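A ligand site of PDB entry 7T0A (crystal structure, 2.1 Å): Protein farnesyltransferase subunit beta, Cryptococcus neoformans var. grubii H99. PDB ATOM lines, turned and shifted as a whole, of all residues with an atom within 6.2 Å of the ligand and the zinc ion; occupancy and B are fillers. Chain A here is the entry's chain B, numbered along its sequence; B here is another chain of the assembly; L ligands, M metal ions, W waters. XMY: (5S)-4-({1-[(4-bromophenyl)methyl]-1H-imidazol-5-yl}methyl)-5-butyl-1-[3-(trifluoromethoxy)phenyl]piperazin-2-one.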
ATOM      1  N   LEU A  84      12.126  -4.865  29.478  1.00  0.00           N
ATOM      2  CA  LEU A  84      11.703  -5.261  28.136  1.00  0.00           C
ATOM      3  C   LEU A  84      10.957  -4.158  27.415  1.00  0.00           C
ATOM      4  O   LEU A  84      10.309  -4.422  26.394  1.00  0.00           O
ATOM      5  CB  LEU A  84      10.841  -6.529  28.211  1.00  0.00           C
ATOM      6  CG  LEU A  84      11.532  -7.765  28.777  1.00  0.00           C
ATOM      7  CD1 LEU A  84      10.547  -8.914  28.902  1.00  0.00           C
ATOM      8  CD2 LEU A  84      12.716  -8.171  27.907  1.00  0.00           C
ATOM      9  N   TRP A  90       9.286  -8.065  20.408  1.00  0.00           N
ATOM     10  CA  TRP A  90       9.627  -9.456  20.733  1.00  0.00           C
ATOM     11  C   TRP A  90       8.561 -10.075  21.623  1.00  0.00           C
ATOM     12  O   TRP A  90       8.255 -11.270  21.491  1.00  0.00           O
ATOM     13  CB  TRP A  90      11.000  -9.522  21.388  1.00  0.00           C
ATOM     14  CG  TRP A  90      12.108  -9.300  20.425  1.00  0.00           C
ATOM     15  CD1 TRP A  90      12.886  -8.180  20.315  1.00  0.00           C
ATOM     16  CD2 TRP A  90      12.571 -10.210  19.416  1.00  0.00           C
ATOM     17  NE1 TRP A  90      13.795  -8.335  19.297  1.00  0.00           N
ATOM     18  CE2 TRP A  90      13.625  -9.579  18.735  1.00  0.00           C
ATOM     19  CE3 TRP A  90      12.182 -11.492  19.029  1.00  0.00           C
ATOM     20  CZ2 TRP A  90      14.304 -10.190  17.679  1.00  0.00           C
ATOM     21  CZ3 TRP A  90      12.870 -12.100  17.993  1.00  0.00           C
ATOM     22  CH2 TRP A  90      13.915 -11.451  17.333  1.00  0.00           C
ATOM     23  N   TRP A  94       6.966 -13.510  20.326  1.00  0.00           N
ATOM     24  CA  TRP A  94       6.973 -14.671  21.212  1.00  0.00           C
ATOM     25  C   TRP A  94       5.565 -15.105  21.561  1.00  0.00           C
ATOM     26  O   TRP A  94       5.315 -16.303  21.770  1.00  0.00           O
ATOM     27  CB  TRP A  94       7.766 -14.356  22.477  1.00  0.00           C
ATOM     28  CG  TRP A  94       9.232 -14.150  22.242  1.00  0.00           C
ATOM     29  CD1 TRP A  94      10.005 -14.732  21.259  1.00  0.00           C
ATOM     30  CD2 TRP A  94      10.115 -13.298  22.986  1.00  0.00           C
ATOM     31  NE1 TRP A  94      11.297 -14.294  21.357  1.00  0.00           N
ATOM     32  CE2 TRP A  94      11.397 -13.412  22.407  1.00  0.00           C
ATOM     33  CE3 TRP A  94       9.944 -12.454  24.079  1.00  0.00           C
ATOM     34  CZ2 TRP A  94      12.504 -12.716  22.890  1.00  0.00           C
ATOM     35  CZ3 TRP A  94      11.046 -11.749  24.562  1.00  0.00           C
ATOM     36  CH2 TRP A  94      12.310 -11.893  23.962  1.00  0.00           C
ATOM     37  N   LEU A 141      16.687  -5.665  15.352  1.00  0.00           N
ATOM     38  CA  LEU A 141      16.051  -6.819  15.975  1.00  0.00           C
ATOM     39  C   LEU A 141      14.542  -6.635  16.112  1.00  0.00           C
ATOM     40  O   LEU A 141      13.792  -7.566  15.748  1.00  0.00           O
ATOM     41  CB  LEU A 141      16.713  -7.138  17.319  1.00  0.00           C
ATOM     42  CG  LEU A 141      17.941  -8.060  17.295  1.00  0.00           C
ATOM     43  CD1 LEU A 141      19.045  -7.521  16.392  1.00  0.00           C
ATOM     44  CD2 LEU A 141      18.476  -8.274  18.709  1.00  0.00           C
ATOM     45  N   TYR A 144      12.856  -7.290  12.646  1.00  0.00           N
ATOM     46  CA  TYR A 144      12.524  -8.681  12.377  1.00  0.00           C
ATOM     47  C   TYR A 144      11.273  -9.107  13.140  1.00  0.00           C
ATOM     48  O   TYR A 144      10.351  -9.694  12.564  1.00  0.00           O
ATOM     49  CB  TYR A 144      13.699  -9.590  12.742  1.00  0.00           C
ATOM     50  CG  TYR A 144      13.343 -11.056  12.891  1.00  0.00           C
ATOM     51  CD1 TYR A 144      13.437 -11.925  11.805  1.00  0.00           C
ATOM     52  CD2 TYR A 144      12.927 -11.582  14.107  1.00  0.00           C
ATOM     53  CE1 TYR A 144      13.099 -13.261  11.928  1.00  0.00           C
ATOM     54  CE2 TYR A 144      12.594 -12.905  14.240  1.00  0.00           C
ATOM     55  CZ  TYR A 144      12.688 -13.751  13.155  1.00  0.00           C
ATOM     56  OH  TYR A 144      12.355 -15.074  13.299  1.00  0.00           O
ATOM     57  N   VAL A 196      26.073 -11.000  14.591  1.00  0.00           N
ATOM     58  CA  VAL A 196      25.332 -11.760  13.603  1.00  0.00           C
ATOM     59  C   VAL A 196      23.827 -11.785  13.853  1.00  0.00           C
ATOM     60  O   VAL A 196      23.078 -12.198  12.965  1.00  0.00           O
ATOM     61  CB  VAL A 196      25.848 -13.216  13.538  1.00  0.00           C
ATOM     62  CG1 VAL A 196      27.254 -13.240  12.954  1.00  0.00           C
ATOM     63  CG2 VAL A 196      25.828 -13.850  14.919  1.00  0.00           C
ATOM     64  N   ARG A 197      23.368 -11.350  15.028  1.00  0.00           N
ATOM     65  CA  ARG A 197      21.928 -11.202  15.225  1.00  0.00           C
ATOM     66  C   ARG A 197      21.372 -10.138  14.296  1.00  0.00           C
ATOM     67  O   ARG A 197      20.294 -10.312  13.709  1.00  0.00           O
ATOM     68  CB  ARG A 197      21.614 -10.838  16.681  1.00  0.00           C
ATOM     69  CG  ARG A 197      22.035 -11.856  17.718  1.00  0.00           C
ATOM     70  CD  ARG A 197      21.860 -11.240  19.105  1.00  0.00           C
ATOM     71  NE  ARG A 197      22.516  -9.939  19.167  1.00  0.00           N
ATOM     72  CZ  ARG A 197      22.244  -9.004  20.071  1.00  0.00           C
ATOM     73  NH1 ARG A 197      21.311  -9.222  20.997  1.00  0.00           N
ATOM     74  NH2 ARG A 197      22.892  -7.847  20.039  1.00  0.00           N
ATOM     75  N   GLY A 198      22.084  -9.016  14.164  1.00  0.00           N
ATOM     76  CA  GLY A 198      21.643  -7.987  13.236  1.00  0.00           C
ATOM     77  C   GLY A 198      21.663  -8.453  11.791  1.00  0.00           C
ATOM     78  O   GLY A 198      20.747  -8.152  11.022  1.00  0.00           O
ATOM     79  N   TYR A 200      21.313 -11.596  10.748  1.00  0.00           N
ATOM     80  CA  TYR A 200      20.206 -12.530  10.567  1.00  0.00           C
ATOM     81  C   TYR A 200      18.877 -11.806  10.434  1.00  0.00           C
ATOM     82  O   TYR A 200      18.111 -12.061   9.500  1.00  0.00           O
ATOM     83  CB  TYR A 200      20.156 -13.514  11.737  1.00  0.00           C
ATOM     84  CG  TYR A 200      18.832 -14.235  11.859  1.00  0.00           C
ATOM     85  CD1 TYR A 200      18.513 -15.277  11.000  1.00  0.00           C
ATOM     86  CD2 TYR A 200      17.905 -13.868  12.823  1.00  0.00           C
ATOM     87  CE1 TYR A 200      17.303 -15.934  11.107  1.00  0.00           C
ATOM     88  CE2 TYR A 200      16.690 -14.516  12.930  1.00  0.00           C
ATOM     89  CZ  TYR A 200      16.390 -15.549  12.072  1.00  0.00           C
ATOM     90  OH  TYR A 200      15.189 -16.203  12.178  1.00  0.00           O
ATOM     91  N   CYS A 201      18.591 -10.890  11.367  1.00  0.00           N
ATOM     92  CA  CYS A 201      17.326 -10.172  11.334  1.00  0.00           C
ATOM     93  C   CYS A 201      17.180  -9.353  10.066  1.00  0.00           C
ATOM     94  O   CYS A 201      16.101  -9.285   9.476  1.00  0.00           O
ATOM     95  CB  CYS A 201      17.204  -9.275  12.570  1.00  0.00           C
ATOM     96  SG  CYS A 201      16.984 -10.180  14.119  1.00  0.00           S
ATOM     97  N   HIS A 266      28.635 -20.123  20.025  1.00  0.00           N
ATOM     98  CA  HIS A 266      27.460 -19.977  20.867  1.00  0.00           C
ATOM     99  C   HIS A 266      26.220 -20.409  20.099  1.00  0.00           C
ATOM    100  O   HIS A 266      26.116 -20.166  18.894  1.00  0.00           O
ATOM    101  CB  HIS A 266      27.317 -18.523  21.349  1.00  0.00           C
ATOM    102  CG  HIS A 266      26.209 -18.316  22.334  1.00  0.00           C
ATOM    103  ND1 HIS A 266      24.913 -18.078  21.946  1.00  0.00           N
ATOM    104  CD2 HIS A 266      26.211 -18.323  23.685  1.00  0.00           C
ATOM    105  CE1 HIS A 266      24.150 -17.934  23.027  1.00  0.00           C
ATOM    106  NE2 HIS A 266      24.918 -18.078  24.088  1.00  0.00           N
ATOM    107  N   GLY A 267      25.291 -21.049  20.812  1.00  0.00           N
ATOM    108  CA  GLY A 267      24.129 -21.613  20.141  1.00  0.00           C
ATOM    109  C   GLY A 267      23.286 -20.586  19.426  1.00  0.00           C
ATOM    110  O   GLY A 267      22.825 -20.818  18.299  1.00  0.00           O
ATOM    111  N   GLY A 268      23.063 -19.426  20.058  1.00  0.00           N
ATOM    112  CA  GLY A 268      22.268 -18.390  19.414  1.00  0.00           C
ATOM    113  C   GLY A 268      22.959 -17.793  18.205  1.00  0.00           C
ATOM    114  O   GLY A 268      22.354 -17.619  17.147  1.00  0.00           O
ATOM    115  N   TYR A 269      24.256 -17.486  18.339  1.00  0.00           N
ATOM    116  CA  TYR A 269      24.982 -16.875  17.221  1.00  0.00           C
ATOM    117  C   TYR A 269      25.299 -17.895  16.136  1.00  0.00           C
ATOM    118  O   TYR A 269      25.454 -17.523  14.969  1.00  0.00           O
ATOM    119  CB  TYR A 269      26.261 -16.222  17.737  1.00  0.00           C
ATOM    120  CG  TYR A 269      25.995 -15.167  18.794  1.00  0.00           C
ATOM    121  CD1 TYR A 269      25.315 -13.998  18.477  1.00  0.00           C
ATOM    122  CD2 TYR A 269      26.426 -15.339  20.098  1.00  0.00           C
ATOM    123  CE1 TYR A 269      25.070 -13.030  19.432  1.00  0.00           C
ATOM    124  CE2 TYR A 269      26.185 -14.381  21.064  1.00  0.00           C
ATOM    125  CZ  TYR A 269      25.505 -13.233  20.725  1.00  0.00           C
ATOM    126  OH  TYR A 269      25.251 -12.270  21.681  1.00  0.00           O
ATOM    127  N   CYS A 272      22.040 -17.841  14.112  1.00  0.00           N
ATOM    128  CA  CYS A 272      21.983 -16.648  13.267  1.00  0.00           C
ATOM    129  C   CYS A 272      22.968 -16.743  12.113  1.00  0.00           C
ATOM    130  O   CYS A 272      22.658 -16.344  10.988  1.00  0.00           O
ATOM    131  CB  CYS A 272      22.261 -15.394  14.102  1.00  0.00           C
ATOM    132  SG  CYS A 272      21.001 -15.043  15.349  1.00  0.00           S
ATOM    133  N   ASP A 323      19.809 -25.581  28.311  1.00  0.00           N
ATOM    134  CA  ASP A 323      18.814 -24.521  28.394  1.00  0.00           C
ATOM    135  C   ASP A 323      17.736 -24.806  27.354  1.00  0.00           C
ATOM    136  O   ASP A 323      18.048 -25.089  26.201  1.00  0.00           O
ATOM    137  CB  ASP A 323      19.442 -23.137  28.149  1.00  0.00           C
ATOM    138  CG  ASP A 323      18.478 -21.990  28.415  1.00  0.00           C
ATOM    139  OD1 ASP A 323      18.916 -20.999  29.035  1.00  0.00           O
ATOM    140  OD2 ASP A 323      17.296 -22.073  28.030  1.00  0.00           O
ATOM    141  N   GLY A 324      16.473 -24.725  27.782  1.00  0.00           N
ATOM    142  CA  GLY A 324      15.378 -25.054  26.880  1.00  0.00           C
ATOM    143  C   GLY A 324      15.309 -24.167  25.655  1.00  0.00           C
ATOM    144  O   GLY A 324      14.866 -24.612  24.592  1.00  0.00           O
ATOM    145  N   CYS A 325      15.752 -22.910  25.773  1.00  0.00           N
ATOM    146  CA  CYS A 325      15.669 -21.999  24.638  1.00  0.00           C
ATOM    147  C   CYS A 325      16.598 -22.405  23.503  1.00  0.00           C
ATOM    148  O   CYS A 325      16.341 -22.048  22.358  1.00  0.00           O
ATOM    149  CB  CYS A 325      15.978 -20.568  25.078  1.00  0.00           C
ATOM    150  SG  CYS A 325      17.718 -20.238  25.442  1.00  0.00           S
ATOM    151  N   TYR A 326      17.655 -23.170  23.790  1.00  0.00           N
ATOM    152  CA  TYR A 326      18.540 -23.654  22.742  1.00  0.00           C
ATOM    153  C   TYR A 326      17.964 -24.838  21.984  1.00  0.00           C
ATOM    154  O   TYR A 326      18.604 -25.327  21.051  1.00  0.00           O
ATOM    155  CB  TYR A 326      19.909 -24.018  23.328  1.00  0.00           C
ATOM    156  CG  TYR A 326      20.650 -22.819  23.869  1.00  0.00           C
ATOM    157  CD1 TYR A 326      21.050 -21.781  23.028  1.00  0.00           C
ATOM    158  CD2 TYR A 326      20.947 -22.701  25.220  1.00  0.00           C
ATOM    159  CE1 TYR A 326      21.726 -20.677  23.526  1.00  0.00           C
ATOM    160  CE2 TYR A 326      21.615 -21.602  25.727  1.00  0.00           C
ATOM    161  CZ  TYR A 326      21.995 -20.594  24.874  1.00  0.00           C
ATOM    162  OH  TYR A 326      22.663 -19.494  25.361  1.00  0.00           O
ATOM    163  N   TRP A 329      17.497 -22.622  19.021  1.00  0.00           N
ATOM    164  CA  TRP A 329      18.752 -22.077  18.482  1.00  0.00           C
ATOM    165  C   TRP A 329      19.620 -23.185  17.914  1.00  0.00           C
ATOM    166  O   TRP A 329      20.065 -23.110  16.754  1.00  0.00           O
ATOM    167  CB  TRP A 329      19.509 -21.313  19.570  1.00  0.00           C
ATOM    168  CG  TRP A 329      18.807 -20.084  20.085  1.00  0.00           C
ATOM    169  CD1 TRP A 329      18.501 -19.801  21.388  1.00  0.00           C
ATOM    170  CD2 TRP A 329      18.321 -18.969  19.309  1.00  0.00           C
ATOM    171  NE1 TRP A 329      17.865 -18.587  21.463  1.00  0.00           N
ATOM    172  CE2 TRP A 329      17.740 -18.056  20.206  1.00  0.00           C
ATOM    173  CE3 TRP A 329      18.330 -18.671  17.947  1.00  0.00           C
ATOM    174  CZ2 TRP A 329      17.170 -16.855  19.792  1.00  0.00           C
ATOM    175  CZ3 TRP A 329      17.760 -17.471  17.523  1.00  0.00           C
ATOM    176  CH2 TRP A 329      17.191 -16.586  18.450  1.00  0.00           C
ATOM    177  N   ASP A 400      13.639 -22.047  31.021  1.00  0.00           N
ATOM    178  CA  ASP A 400      15.021 -22.452  30.796  1.00  0.00           C
ATOM    179  C   ASP A 400      15.291 -23.827  31.399  1.00  0.00           C
ATOM    180  O   ASP A 400      15.643 -24.784  30.696  1.00  0.00           O
ATOM    181  CB  ASP A 400      15.955 -21.386  31.377  1.00  0.00           C
ATOM    182  CG  ASP A 400      17.404 -21.847  31.551  1.00  0.00           C
ATOM    183  OD1 ASP A 400      17.803 -22.919  31.056  1.00  0.00           O
ATOM    184  OD2 ASP A 400      18.160 -21.096  32.209  1.00  0.00           O
ATOM    185  N   ASP A 407       9.063 -17.710  31.005  1.00  0.00           N
ATOM    186  CA  ASP A 407       8.863 -16.412  30.391  1.00  0.00           C
ATOM    187  C   ASP A 407       8.417 -16.608  28.945  1.00  0.00           C
ATOM    188  O   ASP A 407       8.407 -17.724  28.421  1.00  0.00           O
ATOM    189  CB  ASP A 407      10.121 -15.538  30.462  1.00  0.00           C
ATOM    190  CG  ASP A 407      11.360 -16.257  29.964  1.00  0.00           C
ATOM    191  OD1 ASP A 407      11.391 -16.647  28.782  1.00  0.00           O
ATOM    192  OD2 ASP A 407      12.316 -16.407  30.748  1.00  0.00           O
ATOM    193  N   TYR A 409       9.875 -15.603  26.213  1.00  0.00           N
ATOM    194  CA  TYR A 409      10.967 -15.974  25.332  1.00  0.00           C
ATOM    195  C   TYR A 409      11.233 -17.470  25.371  1.00  0.00           C
ATOM    196  O   TYR A 409      11.329 -18.130  24.322  1.00  0.00           O
ATOM    197  CB  TYR A 409      12.235 -15.190  25.701  1.00  0.00           C
ATOM    198  CG  TYR A 409      13.512 -15.825  25.196  1.00  0.00           C
ATOM    199  CD1 TYR A 409      13.847 -15.785  23.843  1.00  0.00           C
ATOM    200  CD2 TYR A 409      14.397 -16.450  26.064  1.00  0.00           C
ATOM    201  CE1 TYR A 409      15.013 -16.351  23.378  1.00  0.00           C
ATOM    202  CE2 TYR A 409      15.567 -17.025  25.609  1.00  0.00           C
ATOM    203  CZ  TYR A 409      15.871 -16.966  24.266  1.00  0.00           C
ATOM    204  OH  TYR A 409      17.042 -17.541  23.821  1.00  0.00           O
ATOM    205  N   HIS A 410      11.358 -18.045  26.577  1.00  0.00           N
ATOM    206  CA  HIS A 410      11.603 -19.475  26.678  1.00  0.00           C
ATOM    207  C   HIS A 410      10.384 -20.291  26.279  1.00  0.00           C
ATOM    208  O   HIS A 410      10.515 -21.432  25.826  1.00  0.00           O
ATOM    209  CB  HIS A 410      12.039 -19.834  28.096  1.00  0.00           C
ATOM    210  CG  HIS A 410      13.423 -19.371  28.428  1.00  0.00           C
ATOM    211  ND1 HIS A 410      13.677 -18.144  29.020  1.00  0.00           N
ATOM    212  CD2 HIS A 410      14.633 -19.955  28.243  1.00  0.00           C
ATOM    213  CE1 HIS A 410      14.981 -18.000  29.190  1.00  0.00           C
ATOM    214  NE2 HIS A 410      15.584 -19.088  28.718  1.00  0.00           N
ATOM    215  N   TYR B 123      23.283  -5.462  26.935  1.00  0.00           N
ATOM    216  CA  TYR B 123      24.033  -5.278  25.704  1.00  0.00           C
ATOM    217  C   TYR B 123      24.460  -3.823  25.537  1.00  0.00           C
ATOM    218  O   TYR B 123      25.545  -3.533  25.016  1.00  0.00           O
ATOM    219  CB  TYR B 123      23.190  -5.705  24.494  1.00  0.00           C
ATOM    220  CG  TYR B 123      23.132  -7.190  24.227  1.00  0.00           C
ATOM    221  CD1 TYR B 123      24.106  -7.815  23.446  1.00  0.00           C
ATOM    222  CD2 TYR B 123      22.108  -7.969  24.733  1.00  0.00           C
ATOM    223  CE1 TYR B 123      24.052  -9.166  23.193  1.00  0.00           C
ATOM    224  CE2 TYR B 123      22.044  -9.324  24.480  1.00  0.00           C
ATOM    225  CZ  TYR B 123      23.019  -9.927  23.710  1.00  0.00           C
ATOM    226  OH  TYR B 123      22.960 -11.270  23.468  1.00  0.00           O
HETATM  227  C10 XMY L   1      19.888 -12.906  25.209  1.00  0.00           C
HETATM  228  C13 XMY L   1      19.519 -15.834  27.034  1.00  0.00           C
HETATM  229  C20 XMY L   1      22.422 -15.114  23.840  1.00  0.00           C
HETATM  230  C21 XMY L   1      22.304 -14.830  22.495  1.00  0.00           C
HETATM  231  C22 XMY L   1      21.357 -15.469  21.737  1.00  0.00           C
HETATM  232  C24 XMY L   1      20.522 -16.405  22.342  1.00  0.00           C
HETATM  233  C26 XMY L   1      17.637 -12.581  21.913  1.00  0.00           C
HETATM  234  C28 XMY L   1      17.823 -12.642  19.493  1.00  0.00           C
HETATM  235  C01 XMY L   1      13.695 -11.878  27.762  1.00  0.00           C
HETATM  236  C02 XMY L   1      14.975 -11.701  26.892  1.00  0.00           C
HETATM  237  C03 XMY L   1      15.855 -12.925  26.911  1.00  0.00           C
HETATM  238  C04 XMY L   1      17.258 -12.652  26.297  1.00  0.00           C
HETATM  239  C05 XMY L   1      17.860 -13.955  25.528  1.00  0.00           C
HETATM  240  C06 XMY L   1      17.436 -13.910  24.100  1.00  0.00           C
HETATM  241  C08 XMY L   1      19.426 -12.416  23.754  1.00  0.00           C
HETATM  242  C12 XMY L   1      19.561 -14.282  26.882  1.00  0.00           C
HETATM  243  C14 XMY L   1      18.504 -16.566  27.592  1.00  0.00           C
HETATM  244  C16 XMY L   1      20.064 -17.948  26.919  1.00  0.00           C
HETATM  245  C18 XMY L   1      21.751 -16.326  25.961  1.00  0.00           C
HETATM  246  C19 XMY L   1      21.592 -16.036  24.446  1.00  0.00           C
HETATM  247  C25 XMY L   1      20.636 -16.680  23.687  1.00  0.00           C
HETATM  248  C27 XMY L   1      18.317 -12.991  20.713  1.00  0.00           C
HETATM  249  C29 XMY L   1      16.650 -11.880  19.424  1.00  0.00           C
HETATM  250  C30 XMY L   1      15.988 -11.483  20.594  1.00  0.00           C
HETATM  251  C31 XMY L   1      16.495 -11.838  21.834  1.00  0.00           C
HETATM  252  C33 XMY L   1      17.916 -12.831  17.008  1.00  0.00           C
HETATM  253  F34 XMY L   1      16.689 -13.437  16.925  1.00  0.00           F
HETATM  254  F35 XMY L   1      17.782 -11.468  16.787  1.00  0.00           F
HETATM  255  F36 XMY L   1      18.726 -13.351  16.047  1.00  0.00           F
HETATM  256  N07 XMY L   1      18.168 -12.972  23.242  1.00  0.00           N
HETATM  257  N11 XMY L   1      19.234 -14.010  25.673  1.00  0.00           N
HETATM  258  N15 XMY L   1      18.851 -17.869  27.518  1.00  0.00           N
HETATM  259  N17 XMY L   1      20.469 -16.699  26.615  1.00  0.00           N
HETATM  260  O09 XMY L   1      20.052 -11.674  23.149  1.00  0.00           O
HETATM  261  O32 XMY L   1      18.533 -13.071  18.293  1.00  0.00           O
HETATM  262 BR23 XMY L   1      21.204 -15.069  19.825  1.00  0.00          BR
HETATM  263 ZN    ZN M   1      17.541 -19.630  27.649  1.00  0.00          ZN
HETATM  264  O   HOH W   1      25.051 -16.078  26.573  1.00  0.00           O
HETATM  265  O   HOH W   2      10.503 -13.140  27.941  1.00  0.00           O
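The zinc ion is bound by N15 of the ligand, NE2 of His 410, SG of Cys 325, OD1 of Asp 323 and OD2 of Asp 323.
The side-chain carboxylate of Asp 407 sits at hydrogen-bond distance from the backbone NH of His 410 (2.6 Å).
SG of Cys 325 lies close to OH of Tyr 409 (3.2 Å).
SG of Cys 272 lies within hydrogen-bond range of O of Gly 268 (3.4 Å).
The side-chain hydroxyl (OH) of Tyr 269 is in hydrogen-bond range of the side-chain hydroxyl (OH) of Tyr 123 of chain B, 3.1 Å away.
SG of Cys 201 sits at hydrogen-bond distance from O of Arg 197 (3.3 Å).
A ring nitrogen (NE2) of His 266 sits at hydrogen-bond distance from the side-chain hydroxyl (OH) of Tyr 326 (3.0 Å).
N of Gly 268 lies within hydrogen-bond range of ND1 of His 266 (3.0 Å).
N of Tyr 409 sits at hydrogen-bond distance from OD1 of Asp 407.
O09 of the ligand is in hydrogen-bond range of OH of Tyr 123 of chain B, at 3.0 Å.
An oxygen (O09) of the ligand sits at hydrogen-bond distance from the guanidinium group of Arg 197.
F35 of the ligand lies close to SG of Cys 201 (3.1 Å).
SG of Cys 272 sits close to F36 of the ligand (2.9 Å).
Leu 84 touches the ligand (CD2 to C01, 3.8 Å).
CZ2 of Trp 90 touches C29 of the ligand, 3.4 Å away.
Trp 94 touches the ligand.
Leu 141 touches the ligand.
Tyr 200 touches the ligand (CD2 to F36, 3.4 Å).
His 266 touches the ligand (CE1 to C20, 3.4 Å).
Gly 268 touches the ligand (CA to BR23, 3.5 Å).
Tyr 269 touches the ligand.
Tyr 326 touches the ligand (OH to C18, 3.4 Å).
Trp 329 touches the ligand.
Tyr 409 touches the ligand.
Within 4 Å of the ligand: Leu 84, Trp 90, Trp 94, Leu 141, Arg 197, Tyr 200, Cys 201, His 266, Gly 268, Tyr 269, Cys 272, Asp 323, Cys 325, Tyr 326, Trp 329, Tyr 409, His 410 and Tyr 123 of chain B.
Along chain A the residues within 4 Å of the ligand span positions 84 to 410.
Tyr 409 touches the zinc ion.
Of the 25 residues printed, 4 come within 4 Å of the zinc ion.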
